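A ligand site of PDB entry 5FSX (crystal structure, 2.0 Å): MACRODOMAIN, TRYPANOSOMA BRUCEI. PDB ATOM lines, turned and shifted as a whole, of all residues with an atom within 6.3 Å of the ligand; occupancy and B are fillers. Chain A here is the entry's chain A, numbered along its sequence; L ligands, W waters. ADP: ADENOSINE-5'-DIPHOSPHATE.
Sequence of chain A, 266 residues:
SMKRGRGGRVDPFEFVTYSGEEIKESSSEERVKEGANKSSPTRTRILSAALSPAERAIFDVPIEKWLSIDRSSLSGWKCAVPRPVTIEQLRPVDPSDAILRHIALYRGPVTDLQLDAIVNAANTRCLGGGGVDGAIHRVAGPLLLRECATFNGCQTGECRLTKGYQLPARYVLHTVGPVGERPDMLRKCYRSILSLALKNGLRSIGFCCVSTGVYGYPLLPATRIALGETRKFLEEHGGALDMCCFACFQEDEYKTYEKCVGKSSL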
ATOM      1  N   GLY A 108       3.149 -21.356  34.258  1.00  0.00           N
ATOM      2  CA  GLY A 108       2.016 -21.220  35.158  1.00  0.00           C
ATOM      3  C   GLY A 108       0.752 -20.717  34.480  1.00  0.00           C
ATOM      4  O   GLY A 108       0.714 -20.493  33.269  1.00  0.00           O
ATOM      5  N   PRO A 109      -0.304 -20.524  35.277  1.00  0.00           N
ATOM      6  CA  PRO A 109      -1.611 -20.175  34.758  1.00  0.00           C
ATOM      7  C   PRO A 109      -1.694 -18.677  34.389  1.00  0.00           C
ATOM      8  O   PRO A 109      -1.101 -17.822  35.049  1.00  0.00           O
ATOM      9  CB  PRO A 109      -2.550 -20.542  35.921  1.00  0.00           C
ATOM     10  CG  PRO A 109      -1.720 -20.312  37.122  1.00  0.00           C
ATOM     11  CD  PRO A 109      -0.313 -20.687  36.743  1.00  0.00           C
ATOM     12  N   VAL A 110      -2.422 -18.391  33.332  1.00  0.00           N
ATOM     13  CA  VAL A 110      -2.493 -17.047  32.798  1.00  0.00           C
ATOM     14  C   VAL A 110      -3.072 -16.075  33.843  1.00  0.00           C
ATOM     15  O   VAL A 110      -2.695 -14.900  33.885  1.00  0.00           O
ATOM     16  CB  VAL A 110      -3.323 -17.036  31.502  1.00  0.00           C
ATOM     17  CG1 VAL A 110      -4.828 -17.085  31.816  1.00  0.00           C
ATOM     18  CG2 VAL A 110      -2.962 -15.825  30.672  1.00  0.00           C
ATOM     19  N   THR A 111      -3.962 -16.583  34.701  1.00  0.00           N
ATOM     20  CA  THR A 111      -4.648 -15.783  35.706  1.00  0.00           C
ATOM     21  C   THR A 111      -3.700 -15.169  36.733  1.00  0.00           C
ATOM     22  O   THR A 111      -4.114 -14.297  37.496  1.00  0.00           O
ATOM     23  CB  THR A 111      -5.670 -16.609  36.485  1.00  0.00           C
ATOM     24  OG1 THR A 111      -5.032 -17.791  36.981  1.00  0.00           O
ATOM     25  CG2 THR A 111      -6.842 -16.983  35.596  1.00  0.00           C
ATOM     26  N   ALA A 121      -9.629 -18.518  26.530  1.00  0.00           N
ATOM     27  CA  ALA A 121      -9.987 -19.441  25.467  1.00  0.00           C
ATOM     28  C   ALA A 121     -11.390 -19.962  25.748  1.00  0.00           C
ATOM     29  O   ALA A 121     -11.580 -20.935  26.489  1.00  0.00           O
ATOM     30  CB  ALA A 121      -8.980 -20.597  25.375  1.00  0.00           C
ATOM     31  N   ALA A 122     -12.369 -19.300  25.158  1.00  0.00           N
ATOM     32  CA  ALA A 122     -13.758 -19.531  25.474  1.00  0.00           C
ATOM     33  C   ALA A 122     -14.424 -20.249  24.336  1.00  0.00           C
ATOM     34  O   ALA A 122     -13.760 -20.668  23.395  1.00  0.00           O
ATOM     35  CB  ALA A 122     -14.460 -18.215  25.742  1.00  0.00           C
ATOM     36  N   GLY A 130     -15.127 -25.040  31.269  1.00  0.00           N
ATOM     37  CA  GLY A 130     -13.996 -25.715  31.893  1.00  0.00           C
ATOM     38  C   GLY A 130     -12.658 -25.114  31.514  1.00  0.00           C
ATOM     39  O   GLY A 130     -12.589 -24.028  30.967  1.00  0.00           O
ATOM     40  N   GLY A 131     -11.585 -25.839  31.823  1.00  0.00           N
ATOM     41  CA  GLY A 131     -10.253 -25.390  31.453  1.00  0.00           C
ATOM     42  C   GLY A 131      -9.953 -23.976  31.921  1.00  0.00           C
ATOM     43  O   GLY A 131     -10.478 -23.525  32.941  1.00  0.00           O
ATOM     44  N   VAL A 132      -9.110 -23.270  31.175  1.00  0.00           N
ATOM     45  CA  VAL A 132      -8.754 -21.890  31.510  1.00  0.00           C
ATOM     46  C   VAL A 132      -9.983 -20.978  31.667  1.00  0.00           C
ATOM     47  O   VAL A 132     -10.021 -20.130  32.548  1.00  0.00           O
ATOM     48  CB  VAL A 132      -7.810 -21.305  30.440  1.00  0.00           C
ATOM     49  CG1 VAL A 132      -8.537 -21.085  29.122  1.00  0.00           C
ATOM     50  CG2 VAL A 132      -7.179 -20.030  30.931  1.00  0.00           C
ATOM     51  N   ASP A 133     -10.978 -21.152  30.794  1.00  0.00           N
ATOM     52  CA  ASP A 133     -12.221 -20.396  30.836  1.00  0.00           C
ATOM     53  C   ASP A 133     -12.880 -20.476  32.209  1.00  0.00           C
ATOM     54  O   ASP A 133     -13.261 -19.451  32.785  1.00  0.00           O
ATOM     55  CB  ASP A 133     -13.174 -20.911  29.742  1.00  0.00           C
ATOM     56  CG  ASP A 133     -14.427 -20.080  29.584  1.00  0.00           C
ATOM     57  OD1 ASP A 133     -14.488 -18.924  30.058  1.00  0.00           O
ATOM     58  OD2 ASP A 133     -15.366 -20.602  28.939  1.00  0.00           O
ATOM     59  N   ALA A 135     -11.426 -21.415  34.975  1.00  0.00           N
ATOM     60  CA  ALA A 135     -10.466 -20.854  35.916  1.00  0.00           C
ATOM     61  C   ALA A 135     -10.515 -19.312  35.978  1.00  0.00           C
ATOM     62  O   ALA A 135     -10.287 -18.721  37.014  1.00  0.00           O
ATOM     63  CB  ALA A 135      -9.085 -21.304  35.571  1.00  0.00           C
ATOM     64  N   ARG A 138     -13.655 -18.391  37.763  1.00  0.00           N
ATOM     65  CA  ARG A 138     -13.480 -18.625  39.193  1.00  0.00           C
ATOM     66  C   ARG A 138     -12.685 -17.530  39.891  1.00  0.00           C
ATOM     67  O   ARG A 138     -13.065 -17.062  40.956  1.00  0.00           O
ATOM     68  CB  ARG A 138     -12.769 -19.954  39.450  1.00  0.00           C
ATOM     69  CG  ARG A 138     -13.692 -21.151  39.528  1.00  0.00           C
ATOM     70  CD  ARG A 138     -13.000 -22.347  40.196  1.00  0.00           C
ATOM     71  NE  ARG A 138     -11.713 -22.684  39.582  1.00  0.00           N
ATOM     72  CZ  ARG A 138     -11.575 -23.338  38.426  1.00  0.00           C
ATOM     73  NH1 ARG A 138     -12.664 -23.730  37.752  1.00  0.00           N
ATOM     74  NH2 ARG A 138     -10.361 -23.603  37.938  1.00  0.00           N
ATOM     75  N   GLY A 177     -11.526 -20.151  19.957  1.00  0.00           N
ATOM     76  CA  GLY A 177     -10.634 -20.842  19.048  1.00  0.00           C
ATOM     77  C   GLY A 177     -11.338 -21.872  18.200  1.00  0.00           C
ATOM     78  O   GLY A 177     -12.419 -22.347  18.551  1.00  0.00           O
ATOM     79  N   PRO A 178     -10.733 -22.254  17.067  1.00  0.00           N
ATOM     80  CA  PRO A 178     -11.401 -23.263  16.249  1.00  0.00           C
ATOM     81  C   PRO A 178     -11.258 -24.622  16.907  1.00  0.00           C
ATOM     82  O   PRO A 178     -10.360 -24.808  17.724  1.00  0.00           O
ATOM     83  CB  PRO A 178     -10.635 -23.202  14.935  1.00  0.00           C
ATOM     84  CG  PRO A 178      -9.248 -22.889  15.376  1.00  0.00           C
ATOM     85  CD  PRO A 178      -9.393 -21.940  16.542  1.00  0.00           C
ATOM     86  N   CYS A 208      -2.825 -17.266  26.735  1.00  0.00           N
ATOM     87  CA  CYS A 208      -2.851 -18.703  27.053  1.00  0.00           C
ATOM     88  C   CYS A 208      -2.771 -19.429  25.719  1.00  0.00           C
ATOM     89  O   CYS A 208      -2.917 -18.798  24.674  1.00  0.00           O
ATOM     90  CB  CYS A 208      -4.118 -19.085  27.841  1.00  0.00           C
ATOM     91  SG  CYS A 208      -5.703 -18.895  26.968  1.00  0.00           S
ATOM     92  N   CYS A 209      -2.527 -20.736  25.730  1.00  0.00           N
ATOM     93  CA  CYS A 209      -2.357 -21.478  24.473  1.00  0.00           C
ATOM     94  C   CYS A 209      -3.700 -21.925  23.886  1.00  0.00           C
ATOM     95  O   CYS A 209      -4.093 -23.075  24.017  1.00  0.00           O
ATOM     96  CB  CYS A 209      -1.446 -22.691  24.689  1.00  0.00           C
ATOM     97  SG  CYS A 209       0.072 -22.232  25.533  1.00  0.00           S
ATOM     98  N   VAL A 210      -4.370 -20.987  23.222  1.00  0.00           N
ATOM     99  CA  VAL A 210      -5.712 -21.182  22.687  1.00  0.00           C
ATOM    100  C   VAL A 210      -5.851 -22.401  21.797  1.00  0.00           C
ATOM    101  O   VAL A 210      -5.001 -22.654  20.956  1.00  0.00           O
ATOM    102  CB  VAL A 210      -6.169 -19.954  21.854  1.00  0.00           C
ATOM    103  CG1 VAL A 210      -7.463 -20.251  21.054  1.00  0.00           C
ATOM    104  CG2 VAL A 210      -6.377 -18.732  22.754  1.00  0.00           C
ATOM    105  N   SER A 211      -6.964 -23.130  21.970  1.00  0.00           N
ATOM    106  CA  SER A 211      -7.392 -24.266  21.152  1.00  0.00           C
ATOM    107  C   SER A 211      -6.575 -25.563  21.329  1.00  0.00           C
ATOM    108  O   SER A 211      -6.936 -26.586  20.758  1.00  0.00           O
ATOM    109  CB  SER A 211      -7.386 -23.888  19.655  1.00  0.00           C
ATOM    110  OG  SER A 211      -8.547 -23.161  19.323  1.00  0.00           O
ATOM    111  N   THR A 212      -5.501 -25.524  22.119  1.00  0.00           N
ATOM    112  CA  THR A 212      -4.594 -26.666  22.207  1.00  0.00           C
ATOM    113  C   THR A 212      -4.927 -27.573  23.383  1.00  0.00           C
ATOM    114  O   THR A 212      -4.223 -28.562  23.606  1.00  0.00           O
ATOM    115  CB  THR A 212      -3.138 -26.232  22.366  1.00  0.00           C
ATOM    116  OG1 THR A 212      -2.967 -25.560  23.618  1.00  0.00           O
ATOM    117  CG2 THR A 212      -2.710 -25.336  21.222  1.00  0.00           C
ATOM    118  N   GLY A 213      -5.962 -27.241  24.135  1.00  0.00           N
ATOM    119  CA  GLY A 213      -6.408 -28.086  25.219  1.00  0.00           C
ATOM    120  C   GLY A 213      -7.395 -29.124  24.710  1.00  0.00           C
ATOM    121  O   GLY A 213      -7.024 -30.023  23.953  1.00  0.00           O
ATOM    122  N   VAL A 214      -8.649 -28.984  25.111  1.00  0.00           N
ATOM    123  CA  VAL A 214      -9.681 -29.905  24.664  1.00  0.00           C
ATOM    124  C   VAL A 214     -10.103 -29.704  23.202  1.00  0.00           C
ATOM    125  O   VAL A 214     -10.652 -30.622  22.594  1.00  0.00           O
ATOM    126  CB  VAL A 214     -10.956 -29.796  25.549  1.00  0.00           C
ATOM    127  CG1 VAL A 214     -10.658 -30.292  26.949  1.00  0.00           C
ATOM    128  CG2 VAL A 214     -11.494 -28.362  25.578  1.00  0.00           C
ATOM    129  N   TYR A 215      -9.857 -28.530  22.613  1.00  0.00           N
ATOM    130  CA  TYR A 215     -10.229 -28.315  21.208  1.00  0.00           C
ATOM    131  C   TYR A 215      -9.253 -29.036  20.251  1.00  0.00           C
ATOM    132  O   TYR A 215      -9.497 -29.120  19.048  1.00  0.00           O
ATOM    133  CB  TYR A 215     -10.296 -26.815  20.887  1.00  0.00           C
ATOM    134  CG  TYR A 215     -11.620 -26.167  21.288  1.00  0.00           C
ATOM    135  CD1 TYR A 215     -12.541 -26.843  22.101  1.00  0.00           C
ATOM    136  CD2 TYR A 215     -11.942 -24.909  20.842  1.00  0.00           C
ATOM    137  CE1 TYR A 215     -13.737 -26.252  22.451  1.00  0.00           C
ATOM    138  CE2 TYR A 215     -13.150 -24.312  21.196  1.00  0.00           C
ATOM    139  CZ  TYR A 215     -14.038 -24.996  21.998  1.00  0.00           C
ATOM    140  OH  TYR A 215     -15.243 -24.409  22.352  1.00  0.00           O
ATOM    141  N   GLY A 216      -8.154 -29.556  20.794  1.00  0.00           N
ATOM    142  CA  GLY A 216      -7.339 -30.534  20.092  1.00  0.00           C
ATOM    143  C   GLY A 216      -6.552 -29.996  18.908  1.00  0.00           C
ATOM    144  O   GLY A 216      -6.321 -30.726  17.936  1.00  0.00           O
ATOM    145  N   ALA A 247       1.737 -17.503  28.654  1.00  0.00           N
ATOM    146  CA  ALA A 247       1.593 -18.281  29.867  1.00  0.00           C
ATOM    147  C   ALA A 247       1.393 -19.744  29.536  1.00  0.00           C
ATOM    148  O   ALA A 247       0.452 -20.147  28.856  1.00  0.00           O
ATOM    149  CB  ALA A 247       0.448 -17.783  30.711  1.00  0.00           C
ATOM    150  N   CYS A 248       2.310 -20.540  30.059  1.00  0.00           N
ATOM    151  CA  CYS A 248       2.360 -21.958  29.749  1.00  0.00           C
ATOM    152  C   CYS A 248       1.996 -22.733  31.013  1.00  0.00           C
ATOM    153  O   CYS A 248       2.769 -22.793  31.961  1.00  0.00           O
ATOM    154  CB  CYS A 248       3.731 -22.324  29.213  1.00  0.00           C
ATOM    155  SG  CYS A 248       4.128 -21.412  27.709  1.00  0.00           S
ATOM    156  N   PHE A 249       0.787 -23.270  30.998  1.00  0.00           N
ATOM    157  CA  PHE A 249       0.182 -23.941  32.138  1.00  0.00           C
ATOM    158  C   PHE A 249       0.792 -25.344  32.315  1.00  0.00           C
ATOM    159  O   PHE A 249       0.822 -25.892  33.407  1.00  0.00           O
ATOM    160  CB  PHE A 249      -1.327 -24.027  31.917  1.00  0.00           C
ATOM    161  CG  PHE A 249      -2.093 -24.577  33.084  1.00  0.00           C
ATOM    162  CD1 PHE A 249      -1.949 -24.055  34.352  1.00  0.00           C
ATOM    163  CD2 PHE A 249      -3.006 -25.603  32.897  1.00  0.00           C
ATOM    164  CE1 PHE A 249      -2.677 -24.541  35.408  1.00  0.00           C
ATOM    165  CE2 PHE A 249      -3.730 -26.098  33.953  1.00  0.00           C
ATOM    166  CZ  PHE A 249      -3.560 -25.565  35.212  1.00  0.00           C
ATOM    167  N   GLN A 250       1.277 -25.888  31.208  1.00  0.00           N
ATOM    168  CA  GLN A 250       1.916 -27.202  31.182  1.00  0.00           C
ATOM    169  C   GLN A 250       3.396 -27.083  30.809  1.00  0.00           C
ATOM    170  O   GLN A 250       3.796 -26.144  30.116  1.00  0.00           O
ATOM    171  CB  GLN A 250       1.197 -28.110  30.197  1.00  0.00           C
ATOM    172  CG  GLN A 250      -0.239 -28.373  30.572  1.00  0.00           C
ATOM    173  CD  GLN A 250      -0.998 -29.018  29.441  1.00  0.00           C
ATOM    174  OE1 GLN A 250      -0.420 -29.687  28.593  1.00  0.00           O
ATOM    175  NE2 GLN A 250      -2.318 -28.818  29.429  1.00  0.00           N
ATOM    176  N   GLU A 253       4.164 -27.062  26.986  1.00  0.00           N
ATOM    177  CA  GLU A 253       3.802 -25.767  26.435  1.00  0.00           C
ATOM    178  C   GLU A 253       4.984 -24.846  26.600  1.00  0.00           C
ATOM    179  O   GLU A 253       5.375 -24.180  25.648  1.00  0.00           O
ATOM    180  CB  GLU A 253       2.552 -25.189  27.131  1.00  0.00           C
ATOM    181  CG  GLU A 253       1.240 -25.862  26.735  1.00  0.00           C
ATOM    182  CD  GLU A 253       0.047 -25.333  27.509  1.00  0.00           C
ATOM    183  OE1 GLU A 253       0.257 -24.528  28.436  1.00  0.00           O
ATOM    184  OE2 GLU A 253      -1.105 -25.722  27.204  1.00  0.00           O
HETATM  185  PB  ADP L   1      -9.458 -24.728  24.521  1.00  0.00           P
HETATM  186  O1B ADP L   1      -8.486 -25.860  24.228  1.00  0.00           O
HETATM  187  O2B ADP L   1      -9.252 -23.515  23.637  1.00  0.00           O
HETATM  188  O3B ADP L   1     -10.908 -25.136  24.633  1.00  0.00           O
HETATM  189  PA  ADP L   1      -8.510 -25.150  27.210  1.00  0.00           P
HETATM  190  O1A ADP L   1      -8.907 -26.596  27.008  1.00  0.00           O
HETATM  191  O2A ADP L   1      -8.842 -24.470  28.514  1.00  0.00           O
HETATM  192  O3A ADP L   1      -9.071 -24.230  26.005  1.00  0.00           O
HETATM  193  O5' ADP L   1      -6.913 -24.994  27.050  1.00  0.00           O
HETATM  194  C5' ADP L   1      -6.342 -23.767  26.582  1.00  0.00           C
HETATM  195  C4' ADP L   1      -5.165 -23.358  27.458  1.00  0.00           C
HETATM  196  O4' ADP L   1      -5.654 -23.161  28.783  1.00  0.00           O
HETATM  197  C3' ADP L   1      -4.078 -24.413  27.545  1.00  0.00           C
HETATM  198  O3' ADP L   1      -2.781 -23.813  27.560  1.00  0.00           O
HETATM  199  C2' ADP L   1      -4.299 -25.069  28.894  1.00  0.00           C
HETATM  200  O2' ADP L   1      -3.076 -25.617  29.408  1.00  0.00           O
HETATM  201  C1' ADP L   1      -4.831 -23.881  29.702  1.00  0.00           C
HETATM  202  N9  ADP L   1      -5.589 -24.293  30.913  1.00  0.00           N
HETATM  203  C8  ADP L   1      -6.427 -25.344  31.009  1.00  0.00           C
HETATM  204  N7  ADP L   1      -6.915 -25.440  32.273  1.00  0.00           N
HETATM  205  C5  ADP L   1      -6.375 -24.449  32.997  1.00  0.00           C
HETATM  206  C6  ADP L   1      -6.477 -23.992  34.393  1.00  0.00           C
HETATM  207  N6  ADP L   1      -7.283 -24.661  35.251  1.00  0.00           N
HETATM  208  N1  ADP L   1      -5.753 -22.920  34.767  1.00  0.00           N
HETATM  209  C2  ADP L   1      -4.950 -22.251  33.898  1.00  0.00           C
HETATM  210  N3  ADP L   1      -4.817 -22.609  32.604  1.00  0.00           N
HETATM  211  C4  ADP L   1      -5.491 -23.686  32.108  1.00  0.00           C
HETATM  212  O   HOH W   1     -11.518 -22.883  28.109  1.00  0.00           O
HETATM  213  O   HOH W   2      -3.286 -20.476  31.426  1.00  0.00           O
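OE2 of Glu 253 is in hydrogen-bond range of O3' of the ligand, 2.6 Å away. An oxygen (O2B) of the ligand is in hydrogen-bond range of the backbone NH of Ser 211 (2.9 Å). The backbone NH (N) of Gly 213 sits at hydrogen-bond distance from an oxygen (O1B) of the ligand (2.9 Å). An oxygen (O2A) of the ligand sits at hydrogen-bond distance from the backbone NH (N) of Val 132. The backbone NH of Val 214 is in hydrogen-bond range of an oxygen (O1A) of the ligand (3.1 Å). The side-chain amide nitrogen (NE2) of Gln 250 is in hydrogen-bond range of an oxygen (O2') of the ligand (3.3 Å). N of Tyr 215 sits at hydrogen-bond distance from O1B of the ligand (3.4 Å).
The side-chain carboxylate (OE1) of Glu 253 sits at hydrogen-bond distance from the backbone NH (N) of Phe 249, at 2.9 Å. The backbone NH (N) of Gln 250 lies within hydrogen-bond range of the side-chain carboxylate (OE1) of Glu 253 (3.3 Å). OE1 of Glu 253 lies close to SG of Cys 209, at 3.7 Å. O of Glu 253 is in hydrogen-bond range of SG of Cys 248. O of Ser 211 lies within hydrogen-bond range of N of Gly 216. The side-chain hydroxyl (OG) of Ser 211 sits at hydrogen-bond distance from the backbone carbonyl oxygen (O) of Pro 178, 2.9 Å away. The backbone carbonyl oxygen of Cys 209 is in hydrogen-bond range of the side-chain hydroxyl of Thr 212 (2.8 Å).
Merely in contact with the ligand: Pro 109, Ala 121, Gly 131, Ala 135, Cys 209, Thr 212 and Phe 249. Hydrophobic or aromatic side chains within 4 Å of the ligand: Pro 109, Ala 121, Val 132, Ala 135, Val 214, Tyr 215 and Phe 249. The nearest printed residue that does not touch the ligand is Val 210 (4.02 Å).
Water W2 lies within hydrogen-bond range of N3 of the ligand (2.9 Å) and N of Val 110 (3.0 Å). Water W1 lies within hydrogen-bond range of O of Ala 121, O2A of the ligand, N of Asp 133 and O of Gly 130.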
